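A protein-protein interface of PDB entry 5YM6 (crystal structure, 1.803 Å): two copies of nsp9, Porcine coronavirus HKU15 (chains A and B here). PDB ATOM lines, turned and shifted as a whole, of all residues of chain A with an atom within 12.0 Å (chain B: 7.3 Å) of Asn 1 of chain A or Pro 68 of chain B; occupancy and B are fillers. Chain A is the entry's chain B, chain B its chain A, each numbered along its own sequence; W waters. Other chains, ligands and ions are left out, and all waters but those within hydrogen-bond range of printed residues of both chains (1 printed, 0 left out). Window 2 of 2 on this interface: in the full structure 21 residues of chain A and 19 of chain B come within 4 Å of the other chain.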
ATOM      1  N   ASN A   1     -23.783   9.203  -0.377  1.00  0.00           N
ATOM      2  CA  ASN A   1     -22.723   9.976  -1.023  1.00  0.00           C
ATOM      3  C   ASN A   1     -22.208   9.321  -2.301  1.00  0.00           C
ATOM      4  O   ASN A   1     -22.268   9.911  -3.388  1.00  0.00           O
ATOM      5  CB  ASN A   1     -21.548  10.205  -0.070  1.00  0.00           C
ATOM      6  CG  ASN A   1     -21.642  11.542   0.668  1.00  0.00           C
ATOM      7  OD1 ASN A   1     -22.437  11.681   1.594  1.00  0.00           O
ATOM      8  ND2 ASN A   1     -20.790  12.504   0.303  1.00  0.00           N
ATOM      9  N   ASN A   2     -21.686   8.105  -2.170  1.00  0.00           N
ATOM     10  CA  ASN A   2     -21.183   7.368  -3.326  1.00  0.00           C
ATOM     11  C   ASN A   2     -22.286   7.170  -4.353  1.00  0.00           C
ATOM     12  O   ASN A   2     -23.217   6.394  -4.133  1.00  0.00           O
ATOM     13  CB  ASN A   2     -20.605   6.010  -2.913  1.00  0.00           C
ATOM     14  CG  ASN A   2     -19.149   6.093  -2.449  1.00  0.00           C
ATOM     15  OD1 ASN A   2     -18.638   7.163  -2.118  1.00  0.00           O
ATOM     16  ND2 ASN A   2     -18.472   4.949  -2.447  1.00  0.00           N
ATOM     17  N   GLU A   3     -22.173   7.857  -5.484  1.00  0.00           N
ATOM     18  CA  GLU A   3     -23.169   7.720  -6.539  1.00  0.00           C
ATOM     19  C   GLU A   3     -22.958   6.418  -7.313  1.00  0.00           C
ATOM     20  O   GLU A   3     -21.827   5.991  -7.544  1.00  0.00           O
ATOM     21  CB  GLU A   3     -23.128   8.924  -7.489  1.00  0.00           C
ATOM     22  CG  GLU A   3     -23.890   8.701  -8.793  1.00  0.00           C
ATOM     23  CD  GLU A   3     -23.695   9.818  -9.799  1.00  0.00           C
ATOM     24  OE1 GLU A   3     -23.857  10.999  -9.422  1.00  0.00           O
ATOM     25  OE2 GLU A   3     -23.372   9.507 -10.969  1.00  0.00           O
ATOM     26  N   LEU A   4     -24.059   5.780  -7.693  1.00  0.00           N
ATOM     27  CA  LEU A   4     -24.004   4.537  -8.445  1.00  0.00           C
ATOM     28  C   LEU A   4     -23.926   4.807  -9.948  1.00  0.00           C
ATOM     29  O   LEU A   4     -24.795   5.472 -10.513  1.00  0.00           O
ATOM     30  CB  LEU A   4     -25.224   3.674  -8.122  1.00  0.00           C
ATOM     31  CG  LEU A   4     -25.533   2.488  -9.037  1.00  0.00           C
ATOM     32  CD1 LEU A   4     -24.713   1.267  -8.655  1.00  0.00           C
ATOM     33  CD2 LEU A   4     -27.025   2.183  -8.998  1.00  0.00           C
ATOM     34  N   CYS A   5     -22.868   4.300 -10.577  1.00  0.00           N
ATOM     35  CA  CYS A   5     -22.705   4.374 -12.027  1.00  0.00           C
ATOM     36  C   CYS A   5     -23.290   3.134 -12.682  1.00  0.00           C
ATOM     37  O   CYS A   5     -22.727   2.040 -12.572  1.00  0.00           O
ATOM     38  CB  CYS A   5     -21.228   4.509 -12.404  1.00  0.00           C
ATOM     39  SG  CYS A   5     -20.430   6.023 -11.832  1.00  0.00           S
ATOM     40  N   ARG A  33     -19.261   1.812 -19.011  1.00  0.00           N
ATOM     41  CA  ARG A  33     -19.401   2.579 -17.777  1.00  0.00           C
ATOM     42  C   ARG A  33     -18.670   3.904 -17.924  1.00  0.00           C
ATOM     43  O   ARG A  33     -17.513   3.935 -18.342  1.00  0.00           O
ATOM     44  CB  ARG A  33     -18.849   1.805 -16.583  1.00  0.00           C
ATOM     45  CG  ARG A  33     -19.079   2.494 -15.246  1.00  0.00           C
ATOM     46  CD  ARG A  33     -17.969   2.166 -14.256  1.00  0.00           C
ATOM     47  NE  ARG A  33     -18.216   2.775 -12.951  1.00  0.00           N
ATOM     48  CZ  ARG A  33     -17.814   3.997 -12.609  1.00  0.00           C
ATOM     49  NH1 ARG A  33     -18.086   4.473 -11.400  1.00  0.00           N
ATOM     50  NH2 ARG A  33     -17.150   4.748 -13.479  1.00  0.00           N
ATOM     51  N   PHE B  19     -31.365   2.647  11.966  1.00  0.00           N
ATOM     52  CA  PHE B  19     -30.510   2.639  13.146  1.00  0.00           C
ATOM     53  C   PHE B  19     -31.304   2.842  14.441  1.00  0.00           C
ATOM     54  O   PHE B  19     -30.818   2.515  15.516  1.00  0.00           O
ATOM     55  CB  PHE B  19     -29.404   3.698  13.009  1.00  0.00           C
ATOM     56  CG  PHE B  19     -28.289   3.291  12.069  1.00  0.00           C
ATOM     57  CD1 PHE B  19     -28.403   3.487  10.697  1.00  0.00           C
ATOM     58  CD2 PHE B  19     -27.134   2.697  12.560  1.00  0.00           C
ATOM     59  CE1 PHE B  19     -27.376   3.095   9.831  1.00  0.00           C
ATOM     60  CE2 PHE B  19     -26.109   2.311  11.704  1.00  0.00           C
ATOM     61  CZ  PHE B  19     -26.232   2.511  10.341  1.00  0.00           C
ATOM     62  N   SER B  44     -34.586   1.770  -1.596  1.00  0.00           N
ATOM     63  CA  SER B  44     -35.510   2.419  -0.681  1.00  0.00           C
ATOM     64  C   SER B  44     -35.387   3.925  -0.851  1.00  0.00           C
ATOM     65  O   SER B  44     -34.355   4.413  -1.306  1.00  0.00           O
ATOM     66  CB  SER B  44     -35.206   2.020   0.766  1.00  0.00           C
ATOM     67  OG  SER B  44     -35.970   2.775   1.690  1.00  0.00           O
ATOM     68  N   LYS B  46     -35.440   5.631   1.798  1.00  0.00           N
ATOM     69  CA  LYS B  46     -34.789   5.962   3.062  1.00  0.00           C
ATOM     70  C   LYS B  46     -33.275   5.811   2.949  1.00  0.00           C
ATOM     71  O   LYS B  46     -32.788   4.829   2.390  1.00  0.00           O
ATOM     72  CB  LYS B  46     -35.326   5.081   4.191  1.00  0.00           C
ATOM     73  CG  LYS B  46     -36.831   5.242   4.426  1.00  0.00           C
ATOM     74  CD  LYS B  46     -37.276   4.522   5.673  1.00  0.00           C
ATOM     75  CE  LYS B  46     -36.642   5.127   6.916  1.00  0.00           C
ATOM     76  NZ  LYS B  46     -36.862   4.274   8.107  1.00  0.00           N
ATOM     77  N   ASP B  47     -32.534   6.785   3.468  1.00  0.00           N
ATOM     78  CA  ASP B  47     -31.079   6.731   3.401  1.00  0.00           C
ATOM     79  C   ASP B  47     -30.442   6.228   4.697  1.00  0.00           C
ATOM     80  O   ASP B  47     -29.219   6.226   4.832  1.00  0.00           O
ATOM     81  CB  ASP B  47     -30.513   8.112   3.030  1.00  0.00           C
ATOM     82  CG  ASP B  47     -30.700   9.152   4.127  1.00  0.00           C
ATOM     83  OD1 ASP B  47     -31.434   8.912   5.118  1.00  0.00           O
ATOM     84  OD2 ASP B  47     -30.094  10.227   3.977  1.00  0.00           O
ATOM     85  N   ASN B  48     -31.253   5.780   5.643  1.00  0.00           N
ATOM     86  CA  ASN B  48     -30.712   5.403   6.943  1.00  0.00           C
ATOM     87  C   ASN B  48     -30.908   3.942   7.332  1.00  0.00           C
ATOM     88  O   ASN B  48     -30.906   3.616   8.513  1.00  0.00           O
ATOM     89  CB  ASN B  48     -31.304   6.301   8.046  1.00  0.00           C
ATOM     90  CG  ASN B  48     -32.796   6.141   8.198  1.00  0.00           C
ATOM     91  OD1 ASN B  48     -33.505   5.932   7.224  1.00  0.00           O
ATOM     92  ND2 ASN B  48     -33.285   6.265   9.431  1.00  0.00           N
ATOM     93  N   LEU B  49     -31.052   3.049   6.356  1.00  0.00           N
ATOM     94  CA  LEU B  49     -31.227   1.635   6.690  1.00  0.00           C
ATOM     95  C   LEU B  49     -29.916   1.013   7.145  1.00  0.00           C
ATOM     96  O   LEU B  49     -28.847   1.363   6.649  1.00  0.00           O
ATOM     97  CB  LEU B  49     -31.782   0.859   5.483  1.00  0.00           C
ATOM     98  CG  LEU B  49     -33.120   1.419   4.976  1.00  0.00           C
ATOM     99  CD1 LEU B  49     -33.611   0.670   3.738  1.00  0.00           C
ATOM    100  CD2 LEU B  49     -34.164   1.340   6.075  1.00  0.00           C
ATOM    101  N   LEU B  65     -26.212  -4.005   5.879  1.00  0.00           N
ATOM    102  CA  LEU B  65     -26.150  -3.294   4.622  1.00  0.00           C
ATOM    103  C   LEU B  65     -24.889  -2.441   4.510  1.00  0.00           C
ATOM    104  O   LEU B  65     -24.430  -1.860   5.487  1.00  0.00           O
ATOM    105  CB  LEU B  65     -27.375  -2.407   4.468  1.00  0.00           C
ATOM    106  CG  LEU B  65     -28.735  -3.108   4.513  1.00  0.00           C
ATOM    107  CD1 LEU B  65     -29.851  -2.079   4.654  1.00  0.00           C
ATOM    108  CD2 LEU B  65     -28.938  -3.965   3.259  1.00  0.00           C
ATOM    109  N   ASP B  66     -24.341  -2.382   3.310  1.00  0.00           N
ATOM    110  CA  ASP B  66     -23.311  -1.391   2.984  1.00  0.00           C
ATOM    111  C   ASP B  66     -23.984  -0.026   2.874  1.00  0.00           C
ATOM    112  O   ASP B  66     -25.210   0.036   2.791  1.00  0.00           O
ATOM    113  CB  ASP B  66     -22.616  -1.759   1.675  1.00  0.00           C
ATOM    114  CG  ASP B  66     -21.583  -2.847   1.850  1.00  0.00           C
ATOM    115  OD1 ASP B  66     -21.126  -3.065   2.986  1.00  0.00           O
ATOM    116  OD2 ASP B  66     -21.233  -3.491   0.839  1.00  0.00           O
ATOM    117  N   PRO B  67     -23.195   1.070   2.860  1.00  0.00           N
ATOM    118  CA  PRO B  67     -23.733   2.436   2.765  1.00  0.00           C
ATOM    119  C   PRO B  67     -24.599   2.687   1.536  1.00  0.00           C
ATOM    120  O   PRO B  67     -24.316   2.131   0.477  1.00  0.00           O
ATOM    121  CB  PRO B  67     -22.467   3.305   2.684  1.00  0.00           C
ATOM    122  CG  PRO B  67     -21.427   2.521   3.353  1.00  0.00           C
ATOM    123  CD  PRO B  67     -21.724   1.081   3.049  1.00  0.00           C
ATOM    124  N   PRO B  68     -25.622   3.543   1.667  1.00  0.00           N
ATOM    125  CA  PRO B  68     -26.520   3.800   0.533  1.00  0.00           C
ATOM    126  C   PRO B  68     -25.815   4.503  -0.618  1.00  0.00           C
ATOM    127  O   PRO B  68     -24.985   5.393  -0.407  1.00  0.00           O
ATOM    128  CB  PRO B  68     -27.626   4.687   1.140  1.00  0.00           C
ATOM    129  CG  PRO B  68     -27.060   5.228   2.398  1.00  0.00           C
ATOM    130  CD  PRO B  68     -26.063   4.216   2.901  1.00  0.00           C
ATOM    131  N   MET B  69     -26.138   4.085  -1.832  1.00  0.00           N
ATOM    132  CA  MET B  69     -25.637   4.726  -3.027  1.00  0.00           C
ATOM    133  C   MET B  69     -26.828   5.385  -3.707  1.00  0.00           C
ATOM    134  O   MET B  69     -27.917   4.830  -3.703  1.00  0.00           O
ATOM    135  CB  MET B  69     -24.961   3.716  -3.961  1.00  0.00           C
ATOM    136  CG  MET B  69     -23.862   2.863  -3.313  1.00  0.00           C
ATOM    137  SD  MET B  69     -23.179   1.673  -4.504  1.00  0.00           S
ATOM    138  CE  MET B  69     -22.302   2.832  -5.554  1.00  0.00           C
ATOM    139  N   ARG B  70     -26.638   6.568  -4.278  1.00  0.00           N
ATOM    140  CA  ARG B  70     -27.757   7.261  -4.909  1.00  0.00           C
ATOM    141  C   ARG B  70     -27.876   6.892  -6.387  1.00  0.00           C
ATOM    142  O   ARG B  70     -26.867   6.735  -7.075  1.00  0.00           O
ATOM    143  CB  ARG B  70     -27.603   8.773  -4.753  1.00  0.00           C
ATOM    144  CG  ARG B  70     -28.909   9.529  -4.858  1.00  0.00           C
ATOM    145  CD  ARG B  70     -28.678  11.005  -5.132  1.00  0.00           C
ATOM    146  NE  ARG B  70     -29.743  11.571  -5.957  1.00  0.00           N
ATOM    147  CZ  ARG B  70     -29.805  12.845  -6.325  1.00  0.00           C
ATOM    148  NH1 ARG B  70     -28.859  13.691  -5.940  1.00  0.00           N
ATOM    149  NH2 ARG B  70     -30.811  13.273  -7.075  1.00  0.00           N
ATOM    150  N   VAL B  82     -34.116   7.665  -4.741  1.00  0.00           N
ATOM    151  CA  VAL B  82     -34.030   6.255  -4.353  1.00  0.00           C
ATOM    152  C   VAL B  82     -32.581   5.837  -4.056  1.00  0.00           C
ATOM    153  O   VAL B  82     -31.652   6.186  -4.781  1.00  0.00           O
ATOM    154  CB  VAL B  82     -34.635   5.341  -5.445  1.00  0.00           C
ATOM    155  CG1 VAL B  82     -33.983   5.594  -6.784  1.00  0.00           C
ATOM    156  CG2 VAL B  82     -34.517   3.873  -5.057  1.00  0.00           C
ATOM    157  N   TYR B  83     -32.396   5.112  -2.960  1.00  0.00           N
ATOM    158  CA  TYR B  83     -31.059   4.674  -2.555  1.00  0.00           C
ATOM    159  C   TYR B  83     -30.907   3.190  -2.816  1.00  0.00           C
ATOM    160  O   TYR B  83     -31.849   2.431  -2.611  1.00  0.00           O
ATOM    161  CB  TYR B  83     -30.817   4.977  -1.077  1.00  0.00           C
ATOM    162  CG  TYR B  83     -30.857   6.453  -0.795  1.00  0.00           C
ATOM    163  CD1 TYR B  83     -29.750   7.255  -1.050  1.00  0.00           C
ATOM    164  CD2 TYR B  83     -32.020   7.056  -0.330  1.00  0.00           C
ATOM    165  CE1 TYR B  83     -29.788   8.620  -0.806  1.00  0.00           C
ATOM    166  CE2 TYR B  83     -32.070   8.423  -0.098  1.00  0.00           C
ATOM    167  CZ  TYR B  83     -30.950   9.194  -0.340  1.00  0.00           C
ATOM    168  OH  TYR B  83     -31.002  10.550  -0.107  1.00  0.00           O
ATOM    169  N   LEU B  84     -29.729   2.785  -3.277  1.00  0.00           N
ATOM    170  CA  LEU B  84     -29.420   1.375  -3.460  1.00  0.00           C
ATOM    171  C   LEU B  84     -28.446   0.955  -2.365  1.00  0.00           C
ATOM    172  O   LEU B  84     -27.469   1.658  -2.099  1.00  0.00           O
ATOM    173  CB  LEU B  84     -28.814   1.112  -4.837  1.00  0.00           C
ATOM    174  CG  LEU B  84     -28.230  -0.273  -5.164  1.00  0.00           C
ATOM    175  CD1 LEU B  84     -29.318  -1.313  -5.287  1.00  0.00           C
ATOM    176  CD2 LEU B  84     -27.394  -0.247  -6.441  1.00  0.00           C
ATOM    177  N   TYR B  85     -28.732  -0.165  -1.715  1.00  0.00           N
ATOM    178  CA  TYR B  85     -27.812  -0.708  -0.721  1.00  0.00           C
ATOM    179  C   TYR B  85     -27.411  -2.103  -1.134  1.00  0.00           C
ATOM    180  O   TYR B  85     -28.284  -2.938  -1.361  1.00  0.00           O
ATOM    181  CB  TYR B  85     -28.428  -0.831   0.661  1.00  0.00           C
ATOM    182  CG  TYR B  85     -29.017   0.393   1.336  1.00  0.00           C
ATOM    183  CD1 TYR B  85     -30.207   0.955   0.888  1.00  0.00           C
ATOM    184  CD2 TYR B  85     -28.436   0.906   2.501  1.00  0.00           C
ATOM    185  CE1 TYR B  85     -30.784   2.046   1.557  1.00  0.00           C
ATOM    186  CE2 TYR B  85     -29.004   1.994   3.174  1.00  0.00           C
ATOM    187  CZ  TYR B  85     -30.174   2.555   2.686  1.00  0.00           C
ATOM    188  OH  TYR B  85     -30.757   3.616   3.340  1.00  0.00           O
ATOM    189  N   PHE B  86     -26.113  -2.394  -1.178  1.00  0.00           N
ATOM    190  CA  PHE B  86     -25.718  -3.787  -1.307  1.00  0.00           C
ATOM    191  C   PHE B  86     -25.627  -4.451   0.064  1.00  0.00           C
ATOM    192  O   PHE B  86     -25.288  -3.806   1.067  1.00  0.00           O
ATOM    193  CB  PHE B  86     -24.376  -3.917  -2.025  1.00  0.00           C
ATOM    194  CG  PHE B  86     -24.470  -3.657  -3.492  1.00  0.00           C
ATOM    195  CD1 PHE B  86     -25.067  -4.590  -4.314  1.00  0.00           C
ATOM    196  CD2 PHE B  86     -23.999  -2.472  -4.033  1.00  0.00           C
ATOM    197  CE1 PHE B  86     -25.173  -4.366  -5.670  1.00  0.00           C
ATOM    198  CE2 PHE B  86     -24.098  -2.237  -5.394  1.00  0.00           C
ATOM    199  CZ  PHE B  86     -24.690  -3.184  -6.210  1.00  0.00           C
HETATM  200  O   HOH W   1     -23.368   6.978   1.933  1.00  0.00           O
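Printed residues of chain B that touch a printed residue of chain A: Pro 68, Met 69, Arg 70 and Leu 84.
Hydrophobic or aromatic side chains of chain B that line the printed part of chain A: Met 69 and Leu 84.
Of the 6 printed residues of chain A, 4 touch a printed residue of chain B.
Hydrophobic or aromatic side chains of chain A that line the printed part of chain B: Leu 4.
No position is printed for both chains.
Of the 8 pairs that touch across the chains among the printed residues, none has its exchanged pair printed and touching as well.
Printed residues of chain B within 4 Å of Asn 1 of chain A: Pro 68.
Printed residues of chain A within 4 Å of Pro 68 of chain B: Asn 1.
No residue of chain A comes within 4 Å of Asp 47 of chain B.
No residue of chain A comes within 4 Å of Pro 67 of chain B.
Of the printed residues of chain A, Met 69 of chain B touches Asn 2, Glu 3 and Leu 4.
No residue of chain A comes within 4 Å of Tyr 85 of chain B.
Of the printed residues of chain B, Glu 3 of chain A touches Met 69 and Arg 70.
Of the printed residues of chain B, Leu 4 of chain A touches Met 69 (3.8 Å), Arg 70 (3.0 Å) and Leu 84 (3.5 Å).
Arg 33 of chain A touches none of the printed residues of chain B.
Pro 68 of chain B touches Asn 1 of chain A.
Met 69 of chain B touches Asn 2 of chain A.
Glu 3 of chain A touches Met 69 of chain B.
O of Arg 70 of chain B touches CA of Glu 3 of chain A, at 3.9 Å.
CE of Met 69 of chain B touches CA of Leu 4 of chain A, 3.8 Å away.
CD2 of Leu 4 of chain A touches CD2 of Leu 84 of chain B (3.5 Å).
The backbone NH (N) of Leu 84 of chain B sits at hydrogen-bond distance from the backbone carbonyl oxygen (O) of Met 69 of chain B.
The backbone NH (N) of Leu 4 of chain A sits at hydrogen-bond distance from the backbone carbonyl oxygen (O) of Arg 70 of chain B, at 3.0 Å.
N of Arg 70 of chain B lies within hydrogen-bond range of O of Asn 2 of chain A, 3.4 Å away.
Water W1 bridges the backbone NH (N) of Asn 1 of chain A (3.2 Å) and the backbone carbonyl oxygen (O) of Pro 68 of chain B (3.3 Å).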
